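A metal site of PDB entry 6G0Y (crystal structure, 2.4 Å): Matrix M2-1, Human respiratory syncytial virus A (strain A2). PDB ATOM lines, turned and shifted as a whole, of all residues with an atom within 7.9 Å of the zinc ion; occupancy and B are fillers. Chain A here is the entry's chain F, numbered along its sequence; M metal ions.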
ATOM      1  N   ASN A   5     -22.157 -17.033   3.766  1.00  0.00           N
ATOM      2  CA  ASN A   5     -21.303 -16.565   2.706  1.00  0.00           C
ATOM      3  C   ASN A   5     -20.682 -15.211   3.046  1.00  0.00           C
ATOM      4  O   ASN A   5     -21.318 -14.356   3.728  1.00  0.00           O
ATOM      5  CB  ASN A   5     -22.128 -16.450   1.423  1.00  0.00           C
ATOM      6  CG  ASN A   5     -22.509 -17.793   0.861  1.00  0.00           C
ATOM      7  OD1 ASN A   5     -21.833 -18.792   1.089  1.00  0.00           O
ATOM      8  ND2 ASN A   5     -23.599 -17.837   0.089  1.00  0.00           N
ATOM      9  N   PRO A   6     -19.442 -14.995   2.577  1.00  0.00           N
ATOM     10  CA  PRO A   6     -18.800 -13.666   2.820  1.00  0.00           C
ATOM     11  C   PRO A   6     -19.636 -12.561   2.212  1.00  0.00           C
ATOM     12  O   PRO A   6     -20.345 -12.803   1.283  1.00  0.00           O
ATOM     13  CB  PRO A   6     -17.438 -13.792   2.144  1.00  0.00           C
ATOM     14  CG  PRO A   6     -17.203 -15.275   2.082  1.00  0.00           C
ATOM     15  CD  PRO A   6     -18.532 -15.916   1.868  1.00  0.00           C
ATOM     16  N   CYS A   7     -19.600 -11.380   2.799  1.00  0.00           N
ATOM     17  CA  CYS A   7     -20.378 -10.251   2.310  1.00  0.00           C
ATOM     18  C   CYS A   7     -19.648  -9.563   1.189  1.00  0.00           C
ATOM     19  O   CYS A   7     -18.499  -9.143   1.335  1.00  0.00           O
ATOM     20  CB  CYS A   7     -20.677  -9.274   3.452  1.00  0.00           C
ATOM     21  SG  CYS A   7     -21.445  -7.738   2.899  1.00  0.00           S
ATOM     22  N   LYS A   8     -20.279  -9.578   0.013  1.00  0.00           N
ATOM     23  CA  LYS A   8     -19.690  -9.007  -1.192  1.00  0.00           C
ATOM     24  C   LYS A   8     -19.104  -7.631  -0.945  1.00  0.00           C
ATOM     25  O   LYS A   8     -17.968  -7.346  -1.323  1.00  0.00           O
ATOM     26  CB  LYS A   8     -20.740  -8.937  -2.304  1.00  0.00           C
ATOM     27  CG  LYS A   8     -20.914 -10.231  -3.084  1.00  0.00           C
ATOM     28  CD  LYS A   8     -21.413  -9.969  -4.493  1.00  0.00           C
ATOM     29  CE  LYS A   8     -20.320 -10.208  -5.515  1.00  0.00           C
ATOM     30  NZ  LYS A   8     -19.546 -11.446  -5.229  1.00  0.00           N
ATOM     31  N   PHE A   9     -19.883  -6.745  -0.322  1.00  0.00           N
ATOM     32  CA  PHE A   9     -19.406  -5.404  -0.035  1.00  0.00           C
ATOM     33  C   PHE A   9     -18.085  -5.500   0.709  1.00  0.00           C
ATOM     34  O   PHE A   9     -17.074  -4.953   0.296  1.00  0.00           O
ATOM     35  CB  PHE A   9     -20.436  -4.642   0.804  1.00  0.00           C
ATOM     36  CG  PHE A   9     -21.730  -4.378   0.096  1.00  0.00           C
ATOM     37  CD1 PHE A   9     -22.808  -5.226   0.262  1.00  0.00           C
ATOM     38  CD2 PHE A   9     -21.866  -3.284  -0.745  1.00  0.00           C
ATOM     39  CE1 PHE A   9     -24.009  -4.988  -0.399  1.00  0.00           C
ATOM     40  CE2 PHE A   9     -23.054  -3.047  -1.410  1.00  0.00           C
ATOM     41  CZ  PHE A   9     -24.128  -3.895  -1.236  1.00  0.00           C
ATOM     42  N   GLU A  10     -18.115  -6.225   1.832  1.00  0.00           N
ATOM     43  CA  GLU A  10     -16.954  -6.454   2.659  1.00  0.00           C
ATOM     44  C   GLU A  10     -15.738  -7.010   1.905  1.00  0.00           C
ATOM     45  O   GLU A  10     -14.600  -6.633   2.203  1.00  0.00           O
ATOM     46  CB  GLU A  10     -17.329  -7.404   3.801  1.00  0.00           C
ATOM     47  CG  GLU A  10     -16.278  -7.486   4.879  1.00  0.00           C
ATOM     48  CD  GLU A  10     -16.236  -6.265   5.779  1.00  0.00           C
ATOM     49  OE1 GLU A  10     -17.070  -5.341   5.629  1.00  0.00           O
ATOM     50  OE2 GLU A  10     -15.334  -6.229   6.636  1.00  0.00           O
ATOM     51  N   ILE A  11     -15.967  -7.906   0.956  1.00  0.00           N
ATOM     52  CA  ILE A  11     -14.870  -8.337   0.055  1.00  0.00           C
ATOM     53  C   ILE A  11     -14.233  -7.167  -0.717  1.00  0.00           C
ATOM     54  O   ILE A  11     -13.077  -7.281  -1.127  1.00  0.00           O
ATOM     55  CB  ILE A  11     -15.278  -9.440  -0.960  1.00  0.00           C
ATOM     56  CG1 ILE A  11     -15.578 -10.752  -0.236  1.00  0.00           C
ATOM     57  CG2 ILE A  11     -14.147  -9.670  -1.965  1.00  0.00           C
ATOM     58  CD1 ILE A  11     -16.418 -11.704  -1.080  1.00  0.00           C
ATOM     59  N   HIS A  14     -15.548  -2.421   3.015  1.00  0.00           N
ATOM     60  CA  HIS A  14     -16.295  -2.355   4.285  1.00  0.00           C
ATOM     61  C   HIS A  14     -17.777  -2.297   4.021  1.00  0.00           C
ATOM     62  O   HIS A  14     -18.221  -1.401   3.305  1.00  0.00           O
ATOM     63  CB  HIS A  14     -15.919  -1.070   5.016  1.00  0.00           C
ATOM     64  CG  HIS A  14     -14.501  -1.048   5.485  1.00  0.00           C
ATOM     65  ND1 HIS A  14     -14.011  -1.885   6.480  1.00  0.00           N
ATOM     66  CD2 HIS A  14     -13.449  -0.278   5.097  1.00  0.00           C
ATOM     67  CE1 HIS A  14     -12.737  -1.629   6.681  1.00  0.00           C
ATOM     68  NE2 HIS A  14     -12.365  -0.660   5.855  1.00  0.00           N
ATOM     69  N   CYS A  15     -18.541  -3.224   4.606  1.00  0.00           N
ATOM     70  CA  CYS A  15     -20.028  -3.229   4.457  1.00  0.00           C
ATOM     71  C   CYS A  15     -20.565  -1.980   5.048  1.00  0.00           C
ATOM     72  O   CYS A  15     -20.094  -1.574   6.096  1.00  0.00           O
ATOM     73  CB  CYS A  15     -20.684  -4.420   5.148  1.00  0.00           C
ATOM     74  SG  CYS A  15     -22.443  -4.738   4.679  1.00  0.00           S
ATOM     75  N   LEU A  16     -21.542  -1.379   4.386  1.00  0.00           N
ATOM     76  CA  LEU A  16     -22.194  -0.164   4.869  1.00  0.00           C
ATOM     77  C   LEU A  16     -23.697  -0.322   5.241  1.00  0.00           C
ATOM     78  O   LEU A  16     -24.376   0.676   5.446  1.00  0.00           O
ATOM     79  CB  LEU A  16     -22.038   0.951   3.818  1.00  0.00           C
ATOM     80  CG  LEU A  16     -20.708   1.507   3.344  1.00  0.00           C
ATOM     81  CD1 LEU A  16     -20.952   2.721   2.459  1.00  0.00           C
ATOM     82  CD2 LEU A  16     -19.787   1.881   4.492  1.00  0.00           C
ATOM     83  N   ASN A  17     -24.177  -1.554   5.310  1.00  0.00           N
ATOM     84  CA  ASN A  17     -25.606  -1.891   5.443  1.00  0.00           C
ATOM     85  C   ASN A  17     -26.113  -2.148   6.892  1.00  0.00           C
ATOM     86  O   ASN A  17     -27.264  -2.514   7.075  1.00  0.00           O
ATOM     87  CB  ASN A  17     -25.937  -3.170   4.651  1.00  0.00           C
ATOM     88  CG  ASN A  17     -25.854  -2.999   3.146  1.00  0.00           C
ATOM     89  OD1 ASN A  17     -26.191  -1.951   2.595  1.00  0.00           O
ATOM     90  ND2 ASN A  17     -25.458  -4.060   2.475  1.00  0.00           N
ATOM     91  N   GLY A  18     -25.265  -1.988   7.898  1.00  0.00           N
ATOM     92  CA  GLY A  18     -25.689  -2.221   9.285  1.00  0.00           C
ATOM     93  C   GLY A  18     -25.984  -3.665   9.682  1.00  0.00           C
ATOM     94  O   GLY A  18     -25.322  -4.583   9.211  1.00  0.00           O
ATOM     95  N   ARG A  20     -29.015  -4.884   9.094  1.00  0.00           N
ATOM     96  CA  ARG A  20     -29.761  -5.270   7.887  1.00  0.00           C
ATOM     97  C   ARG A  20     -29.107  -6.351   7.006  1.00  0.00           C
ATOM     98  O   ARG A  20     -29.824  -7.043   6.288  1.00  0.00           O
ATOM     99  CB  ARG A  20     -30.067  -4.036   6.996  1.00  0.00           C
ATOM    100  CG  ARG A  20     -30.960  -2.971   7.647  1.00  0.00           C
ATOM    101  CD  ARG A  20     -30.682  -1.574   7.101  1.00  0.00           C
ATOM    102  NE  ARG A  20     -31.477  -1.247   5.911  1.00  0.00           N
ATOM    103  CZ  ARG A  20     -31.032  -1.250   4.658  1.00  0.00           C
ATOM    104  NH1 ARG A  20     -29.766  -1.557   4.348  1.00  0.00           N
ATOM    105  NH2 ARG A  20     -31.886  -0.921   3.686  1.00  0.00           N
ATOM    106  N   CYS A  21     -27.771  -6.499   7.071  1.00  0.00           N
ATOM    107  CA  CYS A  21     -27.011  -7.351   6.125  1.00  0.00           C
ATOM    108  C   CYS A  21     -26.941  -8.790   6.595  1.00  0.00           C
ATOM    109  O   CYS A  21     -26.569  -9.077   7.749  1.00  0.00           O
ATOM    110  CB  CYS A  21     -25.585  -6.829   5.859  1.00  0.00           C
ATOM    111  SG  CYS A  21     -24.657  -7.750   4.582  1.00  0.00           S
ATOM    112  N   HIS A  22     -27.307  -9.690   5.688  1.00  0.00           N
ATOM    113  CA  HIS A  22     -27.510 -11.098   6.042  1.00  0.00           C
ATOM    114  C   HIS A  22     -26.264 -11.950   5.854  1.00  0.00           C
ATOM    115  O   HIS A  22     -26.304 -13.140   6.120  1.00  0.00           O
ATOM    116  CB  HIS A  22     -28.729 -11.650   5.287  1.00  0.00           C
ATOM    117  CG  HIS A  22     -30.032 -11.109   5.804  1.00  0.00           C
ATOM    118  ND1 HIS A  22     -31.030 -10.653   4.965  1.00  0.00           N
ATOM    119  CD2 HIS A  22     -30.485 -10.927   7.066  1.00  0.00           C
ATOM    120  CE1 HIS A  22     -32.051 -10.227   5.695  1.00  0.00           C
ATOM    121  NE2 HIS A  22     -31.741 -10.373   6.973  1.00  0.00           N
ATOM    122  N   PHE A  23     -25.161 -11.339   5.431  1.00  0.00           N
ATOM    123  CA  PHE A  23     -23.958 -12.048   5.036  1.00  0.00           C
ATOM    124  C   PHE A  23     -22.843 -11.948   6.051  1.00  0.00           C
ATOM    125  O   PHE A  23     -22.919 -11.165   6.981  1.00  0.00           O
ATOM    126  CB  PHE A  23     -23.469 -11.498   3.717  1.00  0.00           C
ATOM    127  CG  PHE A  23     -24.408 -11.742   2.576  1.00  0.00           C
ATOM    128  CD1 PHE A  23     -24.466 -13.005   1.948  1.00  0.00           C
ATOM    129  CD2 PHE A  23     -25.242 -10.724   2.121  1.00  0.00           C
ATOM    130  CE1 PHE A  23     -25.342 -13.217   0.883  1.00  0.00           C
ATOM    131  CE2 PHE A  23     -26.123 -10.928   1.059  1.00  0.00           C
ATOM    132  CZ  PHE A  23     -26.177 -12.178   0.441  1.00  0.00           C
ATOM    133  N   SER A  24     -21.804 -12.745   5.852  1.00  0.00           N
ATOM    134  CA  SER A  24     -20.734 -12.840   6.867  1.00  0.00           C
ATOM    135  C   SER A  24     -19.722 -11.700   6.808  1.00  0.00           C
ATOM    136  O   SER A  24     -19.155 -11.405   5.749  1.00  0.00           O
ATOM    137  CB  SER A  24     -20.031 -14.171   6.742  1.00  0.00           C
ATOM    138  OG  SER A  24     -19.034 -14.286   7.731  1.00  0.00           O
ATOM    139  N   HIS A  25     -19.472 -11.065   7.952  1.00  0.00           N
ATOM    140  CA  HIS A  25     -18.439 -10.028   8.058  1.00  0.00           C
ATOM    141  C   HIS A  25     -17.330 -10.526   8.958  1.00  0.00           C
ATOM    142  O   HIS A  25     -16.452  -9.786   9.304  1.00  0.00           O
ATOM    143  CB  HIS A  25     -19.030  -8.714   8.580  1.00  0.00           C
ATOM    144  CG  HIS A  25     -20.260  -8.285   7.851  1.00  0.00           C
ATOM    145  ND1 HIS A  25     -21.521  -8.658   8.238  1.00  0.00           N
ATOM    146  CD2 HIS A  25     -20.425  -7.528   6.732  1.00  0.00           C
ATOM    147  CE1 HIS A  25     -22.421  -8.134   7.420  1.00  0.00           C
ATOM    148  NE2 HIS A  25     -21.780  -7.448   6.496  1.00  0.00           N
ATOM    149  N   TRP A  30     -14.290 -17.356   6.800  1.00  0.00           N
ATOM    150  CA  TRP A  30     -14.223 -17.087   5.353  1.00  0.00           C
ATOM    151  C   TRP A  30     -13.346 -18.068   4.630  1.00  0.00           C
ATOM    152  O   TRP A  30     -12.283 -18.443   5.160  1.00  0.00           O
ATOM    153  CB  TRP A  30     -13.705 -15.689   5.047  1.00  0.00           C
ATOM    154  CG  TRP A  30     -14.668 -14.592   5.210  1.00  0.00           C
ATOM    155  CD1 TRP A  30     -15.807 -14.579   6.004  1.00  0.00           C
ATOM    156  CD2 TRP A  30     -14.590 -13.316   4.603  1.00  0.00           C
ATOM    157  NE1 TRP A  30     -16.445 -13.355   5.890  1.00  0.00           N
ATOM    158  CE2 TRP A  30     -15.716 -12.553   5.049  1.00  0.00           C
ATOM    159  CE3 TRP A  30     -13.687 -12.741   3.706  1.00  0.00           C
ATOM    160  CZ2 TRP A  30     -15.964 -11.242   4.616  1.00  0.00           C
ATOM    161  CZ3 TRP A  30     -13.924 -11.424   3.280  1.00  0.00           C
ATOM    162  CH2 TRP A  30     -15.054 -10.682   3.736  1.00  0.00           C
HETATM  163 ZN    ZN M   1     -22.530  -6.921   4.563  1.00  0.00          ZN
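The zinc ion is bound by a ring nitrogen (NE2) of His 25, the side-chain sulfur of Cys 7, the side-chain sulfur of Cys 15 and the side-chain sulfur of Cys 21. The zinc ion has four donor atoms within binding distance.
The nearest printed residue that does not touch the zinc ion is Asn 17 (4.6 Å).
The backbone carbonyl oxygen of Ser 24 lies within hydrogen-bond range of the backbone NH of Cys 7 (3.0 Å). N of Asn 17 sits close to SG of Cys 15, at 3.7 Å. The side-chain sulfur (SG) of Cys 21 lies close to the backbone NH (N) of Phe 23 (3.7 Å). A ring nitrogen (ND1) of His 25 lies close to the backbone carbonyl oxygen (O) of Phe 23 (3.1 Å). The side-chain sulfur (SG) of Cys 7 lies close to the backbone NH (N) of Phe 9 (3.7 Å). The backbone NH of Cys 15 sits at hydrogen-bond distance from the side-chain carboxylate of Glu 10, at 2.8 Å.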
